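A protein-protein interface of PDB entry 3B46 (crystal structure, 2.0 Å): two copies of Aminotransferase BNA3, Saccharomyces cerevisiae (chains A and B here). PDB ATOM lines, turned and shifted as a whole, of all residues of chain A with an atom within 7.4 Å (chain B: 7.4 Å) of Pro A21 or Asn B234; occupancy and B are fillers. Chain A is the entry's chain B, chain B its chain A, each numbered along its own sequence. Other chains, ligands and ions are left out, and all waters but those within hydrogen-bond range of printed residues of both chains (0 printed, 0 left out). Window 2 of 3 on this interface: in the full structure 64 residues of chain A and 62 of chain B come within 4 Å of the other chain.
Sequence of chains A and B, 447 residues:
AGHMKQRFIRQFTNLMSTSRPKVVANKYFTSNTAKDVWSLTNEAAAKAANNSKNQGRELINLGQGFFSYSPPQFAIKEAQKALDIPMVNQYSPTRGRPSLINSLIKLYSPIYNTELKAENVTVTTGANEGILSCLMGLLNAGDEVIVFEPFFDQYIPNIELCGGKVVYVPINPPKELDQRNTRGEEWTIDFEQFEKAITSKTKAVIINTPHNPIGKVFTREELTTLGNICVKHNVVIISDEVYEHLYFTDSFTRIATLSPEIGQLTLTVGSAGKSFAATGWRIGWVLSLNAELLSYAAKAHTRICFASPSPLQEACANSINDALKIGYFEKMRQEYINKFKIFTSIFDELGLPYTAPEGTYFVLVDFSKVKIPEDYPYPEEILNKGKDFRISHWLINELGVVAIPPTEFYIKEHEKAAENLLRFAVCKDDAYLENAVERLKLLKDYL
Of the 23 printed residues of chain B, 6 touch a printed residue of chain A. Hydrophobic or aromatic side chains of chain B that line the printed part of chain A: Val B236 and Leu B265. Of the 4 printed residues of chain A, 4 touch a printed residue of chain B. Hydrophobic or aromatic side chains of chain A that line the printed part of chain B: Pro A21 and Val A23. Among the printed residues, 9 pairs touch across the chains. Among the printed residues, no Asp or Glu carboxylate lies within 4 Å of a Lys or Arg side-chain nitrogen of the other chain.
NZ of Lys B203 sits at hydrogen-bond distance from O of Val A24 (2.7 Å). O of Lys A22 is in hydrogen-bond range of ND2 of Asn B234.
Among the printed residues, pairs that only touch across the chains: Pro A21 with Asn B234 (2.9 Å), Pro A21 with Leu B265 (3.6 Å), Val A23 with Lys B203 (3.6 Å), Val A23 with Val B236 (3.6 Å), Pro A21 with Gln B264 (3.8 Å), Pro A21 with Asn B290 (3.9 Å) and Val A23 with Asn B234 (3.9 Å).
No position is printed for both chains. Of the 9 pairs that touch across the chains among the printed residues, none has its exchanged pair printed and touching as well.
Of the printed residues of chain B, Pro A21 touches Asn B234 (2.9 Å), Gln B264 (3.8 Å), Leu B265 (3.6 Å) and Asn B290 (3.9 Å). Of the printed residues of chain B, Lys A22 touches Asn B234. Of the printed residues of chain B, Val A23 touches Lys B203, Asn B234 and Val B236. Of the printed residues of chain B, Val A24 touches Lys B203 (2.7 Å). Lys B232 touches none of the printed residues of chain A. Of the printed residues of chain A, Asn B234 touches Pro A21, Lys A22 and Val A23. Printed residues of chain A within 4 Å of Val B236: Val A23 (3.6 Å). Printed residues of chain A within 4 Å of Leu B265: Pro A21 (3.6 Å). The nearest residue of chain B that does not touch Pro A21 is Glu B261 (5.2 Å). The nearest printed residue of chain B that does not touch Val A24 is Asn B234 (5.9 Å).
The backbone carbonyl oxygen (O) of Lys B203 sits at hydrogen-bond distance from the backbone NH (N) of Val B236 (3.2 Å). The backbone NH (N) of Ile B237 is in hydrogen-bond range of the backbone carbonyl oxygen (O) of Leu B265 (2.6 Å). O of Gln B264 is in hydrogen-bond range of ND2 of Asn B290, 2.8 Å away. N of Glu B292 sits at hydrogen-bond distance from OD1 of Asn B290, 3.1 Å away. The side-chain amide oxygen (OD1) of Asn B290 lies within hydrogen-bond range of the backbone NH (N) of Leu B293, 3.2 Å away.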
ATOM      1  N   PRO A  21     -13.420 -22.644 -15.214  1.00  0.00           N
ATOM      2  CA  PRO A  21     -12.820 -21.333 -15.523  1.00  0.00           C
ATOM      3  C   PRO A  21     -12.203 -21.308 -16.917  1.00  0.00           C
ATOM      4  O   PRO A  21     -12.654 -22.018 -17.816  1.00  0.00           O
ATOM      5  CB  PRO A  21     -11.766 -21.079 -14.458  1.00  0.00           C
ATOM      6  CG  PRO A  21     -12.334 -21.847 -13.289  1.00  0.00           C
ATOM      7  CD  PRO A  21     -12.916 -23.123 -13.914  1.00  0.00           C
ATOM      8  N   LYS A  22     -11.175 -20.486 -17.092  1.00  0.00           N
ATOM      9  CA  LYS A  22     -10.504 -20.382 -18.377  1.00  0.00           C
ATOM     10  C   LYS A  22      -9.009 -20.505 -18.151  1.00  0.00           C
ATOM     11  O   LYS A  22      -8.316 -19.497 -18.024  1.00  0.00           O
ATOM     12  CB  LYS A  22     -10.801 -19.029 -19.032  1.00  0.00           C
ATOM     13  CG  LYS A  22     -12.266 -18.652 -19.049  1.00  0.00           C
ATOM     14  CD  LYS A  22     -12.521 -17.429 -19.919  1.00  0.00           C
ATOM     15  CE  LYS A  22     -14.016 -17.117 -19.988  1.00  0.00           C
ATOM     16  NZ  LYS A  22     -14.335 -16.056 -20.989  1.00  0.00           N
ATOM     17  N   VAL A  23      -8.512 -21.734 -18.080  1.00  0.00           N
ATOM     18  CA  VAL A  23      -7.083 -21.939 -17.885  1.00  0.00           C
ATOM     19  C   VAL A  23      -6.441 -22.332 -19.202  1.00  0.00           C
ATOM     20  O   VAL A  23      -6.935 -23.204 -19.913  1.00  0.00           O
ATOM     21  CB  VAL A  23      -6.798 -23.039 -16.831  1.00  0.00           C
ATOM     22  CG1 VAL A  23      -5.329 -23.437 -16.874  1.00  0.00           C
ATOM     23  CG2 VAL A  23      -7.141 -22.524 -15.448  1.00  0.00           C
ATOM     24  N   VAL A  24      -5.342 -21.676 -19.534  1.00  0.00           N
ATOM     25  CA  VAL A  24      -4.650 -21.993 -20.768  1.00  0.00           C
ATOM     26  C   VAL A  24      -3.809 -23.245 -20.554  1.00  0.00           C
ATOM     27  O   VAL A  24      -2.780 -23.196 -19.883  1.00  0.00           O
ATOM     28  CB  VAL A  24      -3.718 -20.856 -21.203  1.00  0.00           C
ATOM     29  CG1 VAL A  24      -2.984 -21.254 -22.467  1.00  0.00           C
ATOM     30  CG2 VAL A  24      -4.515 -19.586 -21.417  1.00  0.00           C
ATOM     31  N   ILE B 198       2.225 -14.532  -7.150  1.00  0.00           N
ATOM     32  CA  ILE B 198       1.332 -14.822  -8.259  1.00  0.00           C
ATOM     33  C   ILE B 198       1.461 -13.707  -9.280  1.00  0.00           C
ATOM     34  O   ILE B 198       1.420 -12.526  -8.928  1.00  0.00           O
ATOM     35  CB  ILE B 198      -0.141 -14.878  -7.813  1.00  0.00           C
ATOM     36  CG1 ILE B 198      -0.324 -15.953  -6.737  1.00  0.00           C
ATOM     37  CG2 ILE B 198      -1.035 -15.141  -9.024  1.00  0.00           C
ATOM     38  CD1 ILE B 198      -1.769 -16.129  -6.262  1.00  0.00           C
ATOM     39  N   THR B 202       1.718 -17.048 -13.855  1.00  0.00           N
ATOM     40  CA  THR B 202       1.468 -18.129 -12.905  1.00  0.00           C
ATOM     41  C   THR B 202       0.384 -19.097 -13.338  1.00  0.00           C
ATOM     42  O   THR B 202      -0.802 -18.766 -13.320  1.00  0.00           O
ATOM     43  CB  THR B 202       1.089 -17.573 -11.522  1.00  0.00           C
ATOM     44  OG1 THR B 202       2.231 -16.939 -10.930  1.00  0.00           O
ATOM     45  CG2 THR B 202       0.616 -18.689 -10.616  1.00  0.00           C
ATOM     46  N   LYS B 203       0.785 -20.309 -13.708  1.00  0.00           N
ATOM     47  CA  LYS B 203      -0.184 -21.302 -14.143  1.00  0.00           C
ATOM     48  C   LYS B 203      -0.755 -22.141 -12.998  1.00  0.00           C
ATOM     49  O   LYS B 203      -1.930 -22.514 -13.014  1.00  0.00           O
ATOM     50  CB  LYS B 203       0.440 -22.216 -15.202  1.00  0.00           C
ATOM     51  CG  LYS B 203      -0.438 -23.382 -15.623  1.00  0.00           C
ATOM     52  CD  LYS B 203      -1.810 -22.941 -16.116  1.00  0.00           C
ATOM     53  CE  LYS B 203      -1.693 -21.933 -17.244  1.00  0.00           C
ATOM     54  NZ  LYS B 203      -0.780 -22.398 -18.323  1.00  0.00           N
ATOM     55  N   ALA B 204       0.060 -22.424 -11.991  1.00  0.00           N
ATOM     56  CA  ALA B 204      -0.433 -23.240 -10.900  1.00  0.00           C
ATOM     57  C   ALA B 204       0.432 -23.206  -9.660  1.00  0.00           C
ATOM     58  O   ALA B 204       1.506 -22.620  -9.642  1.00  0.00           O
ATOM     59  CB  ALA B 204      -0.606 -24.684 -11.380  1.00  0.00           C
ATOM     60  N   ASN B 228      -9.497 -19.748  -2.218  1.00  0.00           N
ATOM     61  CA  ASN B 228     -10.108 -18.530  -2.735  1.00  0.00           C
ATOM     62  C   ASN B 228      -9.131 -17.603  -3.442  1.00  0.00           C
ATOM     63  O   ASN B 228      -9.505 -16.946  -4.415  1.00  0.00           O
ATOM     64  CB  ASN B 228     -10.838 -17.799  -1.617  1.00  0.00           C
ATOM     65  CG  ASN B 228     -12.056 -18.559  -1.150  1.00  0.00           C
ATOM     66  OD1 ASN B 228     -12.832 -19.069  -1.966  1.00  0.00           O
ATOM     67  ND2 ASN B 228     -12.237 -18.645   0.160  1.00  0.00           N
ATOM     68  N   ILE B 229      -7.883 -17.550  -2.979  1.00  0.00           N
ATOM     69  CA  ILE B 229      -6.895 -16.703  -3.636  1.00  0.00           C
ATOM     70  C   ILE B 229      -6.754 -17.177  -5.078  1.00  0.00           C
ATOM     71  O   ILE B 229      -6.853 -16.388  -6.027  1.00  0.00           O
ATOM     72  CB  ILE B 229      -5.506 -16.798  -2.970  1.00  0.00           C
ATOM     73  CG1 ILE B 229      -5.591 -16.336  -1.514  1.00  0.00           C
ATOM     74  CG2 ILE B 229      -4.505 -15.969  -3.763  1.00  0.00           C
ATOM     75  CD1 ILE B 229      -4.253 -16.114  -0.835  1.00  0.00           C
ATOM     76  N   CYS B 230      -6.529 -18.480  -5.233  1.00  0.00           N
ATOM     77  CA  CYS B 230      -6.366 -19.080  -6.549  1.00  0.00           C
ATOM     78  C   CYS B 230      -7.583 -18.915  -7.475  1.00  0.00           C
ATOM     79  O   CYS B 230      -7.407 -18.752  -8.686  1.00  0.00           O
ATOM     80  CB  CYS B 230      -6.015 -20.570  -6.407  1.00  0.00           C
ATOM     81  SG  CYS B 230      -4.437 -20.906  -5.569  1.00  0.00           S
ATOM     82  N   VAL B 231      -8.809 -18.975  -6.943  1.00  0.00           N
ATOM     83  CA  VAL B 231      -9.962 -18.807  -7.831  1.00  0.00           C
ATOM     84  C   VAL B 231     -10.015 -17.342  -8.258  1.00  0.00           C
ATOM     85  O   VAL B 231     -10.442 -17.023  -9.374  1.00  0.00           O
ATOM     86  CB  VAL B 231     -11.323 -19.271  -7.179  1.00  0.00           C
ATOM     87  CG1 VAL B 231     -11.085 -19.809  -5.801  1.00  0.00           C
ATOM     88  CG2 VAL B 231     -12.343 -18.139  -7.160  1.00  0.00           C
ATOM     89  N   LYS B 232      -9.543 -16.464  -7.374  1.00  0.00           N
ATOM     90  CA  LYS B 232      -9.496 -15.035  -7.656  1.00  0.00           C
ATOM     91  C   LYS B 232      -8.462 -14.774  -8.745  1.00  0.00           C
ATOM     92  O   LYS B 232      -8.699 -13.971  -9.649  1.00  0.00           O
ATOM     93  CB  LYS B 232      -9.138 -14.250  -6.383  1.00  0.00           C
ATOM     94  CG  LYS B 232     -10.329 -13.953  -5.469  1.00  0.00           C
ATOM     95  CD  LYS B 232     -11.357 -15.092  -5.472  1.00  0.00           C
ATOM     96  CE  LYS B 232     -12.562 -14.807  -4.577  1.00  0.00           C
ATOM     97  NZ  LYS B 232     -12.209 -14.793  -3.127  1.00  0.00           N
ATOM     98  N   HIS B 233      -7.327 -15.467  -8.665  1.00  0.00           N
ATOM     99  CA  HIS B 233      -6.249 -15.318  -9.653  1.00  0.00           C
ATOM    100  C   HIS B 233      -6.251 -16.400 -10.749  1.00  0.00           C
ATOM    101  O   HIS B 233      -5.314 -16.491 -11.550  1.00  0.00           O
ATOM    102  CB  HIS B 233      -4.890 -15.301  -8.946  1.00  0.00           C
ATOM    103  CG  HIS B 233      -4.680 -14.103  -8.073  1.00  0.00           C
ATOM    104  ND1 HIS B 233      -3.692 -13.171  -8.311  1.00  0.00           N
ATOM    105  CD2 HIS B 233      -5.349 -13.671  -6.978  1.00  0.00           C
ATOM    106  CE1 HIS B 233      -3.762 -12.216  -7.402  1.00  0.00           C
ATOM    107  NE2 HIS B 233      -4.760 -12.495  -6.582  1.00  0.00           N
ATOM    108  N   ASN B 234      -7.314 -17.204 -10.769  1.00  0.00           N
ATOM    109  CA  ASN B 234      -7.503 -18.284 -11.741  1.00  0.00           C
ATOM    110  C   ASN B 234      -6.258 -19.175 -11.858  1.00  0.00           C
ATOM    111  O   ASN B 234      -5.788 -19.473 -12.957  1.00  0.00           O
ATOM    112  CB  ASN B 234      -7.869 -17.694 -13.105  1.00  0.00           C
ATOM    113  CG  ASN B 234      -8.614 -18.680 -13.995  1.00  0.00           C
ATOM    114  OD1 ASN B 234      -9.577 -19.323 -13.568  1.00  0.00           O
ATOM    115  ND2 ASN B 234      -8.182 -18.789 -15.245  1.00  0.00           N
ATOM    116  N   VAL B 235      -5.743 -19.598 -10.709  1.00  0.00           N
ATOM    117  CA  VAL B 235      -4.561 -20.446 -10.655  1.00  0.00           C
ATOM    118  C   VAL B 235      -4.939 -21.876 -10.278  1.00  0.00           C
ATOM    119  O   VAL B 235      -5.590 -22.112  -9.262  1.00  0.00           O
ATOM    120  CB  VAL B 235      -3.551 -19.892  -9.648  1.00  0.00           C
ATOM    121  CG1 VAL B 235      -2.357 -20.828  -9.526  1.00  0.00           C
ATOM    122  CG2 VAL B 235      -3.101 -18.509 -10.096  1.00  0.00           C
ATOM    123  N   VAL B 236      -4.539 -22.823 -11.116  1.00  0.00           N
ATOM    124  CA  VAL B 236      -4.830 -24.232 -10.883  1.00  0.00           C
ATOM    125  C   VAL B 236      -4.148 -24.736  -9.618  1.00  0.00           C
ATOM    126  O   VAL B 236      -2.986 -24.427  -9.368  1.00  0.00           O
ATOM    127  CB  VAL B 236      -4.363 -25.091 -12.064  1.00  0.00           C
ATOM    128  CG1 VAL B 236      -4.627 -26.570 -11.778  1.00  0.00           C
ATOM    129  CG2 VAL B 236      -5.081 -24.654 -13.329  1.00  0.00           C
ATOM    130  N   ILE B 237      -4.893 -25.496  -8.818  1.00  0.00           N
ATOM    131  CA  ILE B 237      -4.363 -26.073  -7.581  1.00  0.00           C
ATOM    132  C   ILE B 237      -4.065 -27.559  -7.778  1.00  0.00           C
ATOM    133  O   ILE B 237      -4.980 -28.362  -7.932  1.00  0.00           O
ATOM    134  CB  ILE B 237      -5.371 -25.963  -6.411  1.00  0.00           C
ATOM    135  CG1 ILE B 237      -5.710 -24.487  -6.141  1.00  0.00           C
ATOM    136  CG2 ILE B 237      -4.784 -26.590  -5.145  1.00  0.00           C
ATOM    137  CD1 ILE B 237      -6.751 -24.291  -5.054  1.00  0.00           C
ATOM    138  N   PRO B 260     -17.112 -24.827  -4.478  1.00  0.00           N
ATOM    139  CA  PRO B 260     -17.335 -25.041  -5.912  1.00  0.00           C
ATOM    140  C   PRO B 260     -16.301 -24.456  -6.878  1.00  0.00           C
ATOM    141  O   PRO B 260     -15.835 -25.150  -7.788  1.00  0.00           O
ATOM    142  CB  PRO B 260     -18.726 -24.455  -6.119  1.00  0.00           C
ATOM    143  CG  PRO B 260     -19.426 -24.903  -4.881  1.00  0.00           C
ATOM    144  CD  PRO B 260     -18.403 -24.696  -3.772  1.00  0.00           C
ATOM    145  N   GLU B 261     -15.948 -23.189  -6.682  1.00  0.00           N
ATOM    146  CA  GLU B 261     -14.979 -22.514  -7.541  1.00  0.00           C
ATOM    147  C   GLU B 261     -13.569 -23.077  -7.370  1.00  0.00           C
ATOM    148  O   GLU B 261     -12.825 -23.196  -8.341  1.00  0.00           O
ATOM    149  CB  GLU B 261     -14.984 -20.999  -7.269  1.00  0.00           C
ATOM    150  CG  GLU B 261     -16.346 -20.327  -7.516  1.00  0.00           C
ATOM    151  CD  GLU B 261     -17.376 -20.635  -6.425  1.00  0.00           C
ATOM    152  OE1 GLU B 261     -18.593 -20.626  -6.726  1.00  0.00           O
ATOM    153  OE2 GLU B 261     -16.967 -20.870  -5.263  1.00  0.00           O
ATOM    154  N   ILE B 262     -13.207 -23.413  -6.135  1.00  0.00           N
ATOM    155  CA  ILE B 262     -11.898 -23.984  -5.840  1.00  0.00           C
ATOM    156  C   ILE B 262     -11.805 -25.369  -6.464  1.00  0.00           C
ATOM    157  O   ILE B 262     -10.809 -25.702  -7.101  1.00  0.00           O
ATOM    158  CB  ILE B 262     -11.683 -24.111  -4.330  1.00  0.00           C
ATOM    159  CG1 ILE B 262     -11.467 -22.725  -3.732  1.00  0.00           C
ATOM    160  CG2 ILE B 262     -10.498 -25.026  -4.039  1.00  0.00           C
ATOM    161  CD1 ILE B 262     -11.594 -22.688  -2.234  1.00  0.00           C
ATOM    162  N   GLY B 263     -12.860 -26.160  -6.274  1.00  0.00           N
ATOM    163  CA  GLY B 263     -12.919 -27.510  -6.813  1.00  0.00           C
ATOM    164  C   GLY B 263     -12.765 -27.547  -8.324  1.00  0.00           C
ATOM    165  O   GLY B 263     -12.205 -28.499  -8.879  1.00  0.00           O
ATOM    166  N   GLN B 264     -13.259 -26.508  -8.991  1.00  0.00           N
ATOM    167  CA  GLN B 264     -13.166 -26.418 -10.440  1.00  0.00           C
ATOM    168  C   GLN B 264     -11.770 -26.101 -10.924  1.00  0.00           C
ATOM    169  O   GLN B 264     -11.493 -26.191 -12.117  1.00  0.00           O
ATOM    170  CB  GLN B 264     -14.143 -25.371 -10.955  1.00  0.00           C
ATOM    171  CG  GLN B 264     -15.507 -25.939 -11.093  1.00  0.00           C
ATOM    172  CD  GLN B 264     -15.588 -26.885 -12.251  1.00  0.00           C
ATOM    173  OE1 GLN B 264     -16.167 -27.963 -12.150  1.00  0.00           O
ATOM    174  NE2 GLN B 264     -15.019 -26.482 -13.374  1.00  0.00           N
ATOM    175  N   LEU B 265     -10.893 -25.735  -9.993  1.00  0.00           N
ATOM    176  CA  LEU B 265      -9.508 -25.419 -10.317  1.00  0.00           C
ATOM    177  C   LEU B 265      -8.522 -26.366  -9.613  1.00  0.00           C
ATOM    178  O   LEU B 265      -7.313 -26.156  -9.653  1.00  0.00           O
ATOM    179  CB  LEU B 265      -9.193 -23.969  -9.928  1.00  0.00           C
ATOM    180  CG  LEU B 265      -9.528 -22.888 -10.962  1.00  0.00           C
ATOM    181  CD1 LEU B 265     -10.363 -21.797 -10.318  1.00  0.00           C
ATOM    182  CD2 LEU B 265      -8.233 -22.322 -11.532  1.00  0.00           C
ATOM    183  N   ASN B 290     -13.553 -30.620 -12.253  1.00  0.00           N
ATOM    184  CA  ASN B 290     -13.485 -29.976 -13.566  1.00  0.00           C
ATOM    185  C   ASN B 290     -12.895 -30.965 -14.564  1.00  0.00           C
ATOM    186  O   ASN B 290     -11.678 -31.005 -14.767  1.00  0.00           O
ATOM    187  CB  ASN B 290     -12.601 -28.727 -13.491  1.00  0.00           C
ATOM    188  CG  ASN B 290     -12.507 -27.999 -14.813  1.00  0.00           C
ATOM    189  OD1 ASN B 290     -12.886 -28.530 -15.855  1.00  0.00           O
ATOM    190  ND2 ASN B 290     -11.984 -26.777 -14.782  1.00  0.00           N
ATOM    191  N   GLU B 292     -12.615 -31.031 -17.727  1.00  0.00           N
ATOM    192  CA  GLU B 292     -11.806 -30.524 -18.836  1.00  0.00           C
ATOM    193  C   GLU B 292     -10.387 -30.277 -18.344  1.00  0.00           C
ATOM    194  O   GLU B 292      -9.407 -30.521 -19.056  1.00  0.00           O
ATOM    195  CB  GLU B 292     -12.386 -29.227 -19.399  1.00  0.00           C
ATOM    196  CG  GLU B 292     -11.722 -28.786 -20.698  1.00  0.00           C
ATOM    197  CD  GLU B 292     -12.244 -27.444 -21.206  1.00  0.00           C
ATOM    198  OE1 GLU B 292     -13.455 -27.350 -21.520  1.00  0.00           O
ATOM    199  OE2 GLU B 292     -11.442 -26.485 -21.287  1.00  0.00           O
ATOM    200  N   LEU B 293     -10.283 -29.782 -17.120  1.00  0.00           N
ATOM    201  CA  LEU B 293      -8.986 -29.533 -16.519  1.00  0.00           C
ATOM    202  C   LEU B 293      -8.239 -30.883 -16.459  1.00  0.00           C
ATOM    203  O   LEU B 293      -7.073 -30.976 -16.822  1.00  0.00           O
ATOM    204  CB  LEU B 293      -9.172 -28.990 -15.101  1.00  0.00           C
ATOM    205  CG  LEU B 293      -8.267 -27.891 -14.543  1.00  0.00           C
ATOM    206  CD1 LEU B 293      -8.147 -28.088 -13.037  1.00  0.00           C
ATOM    207  CD2 LEU B 293      -6.904 -27.926 -15.184  1.00  0.00           C
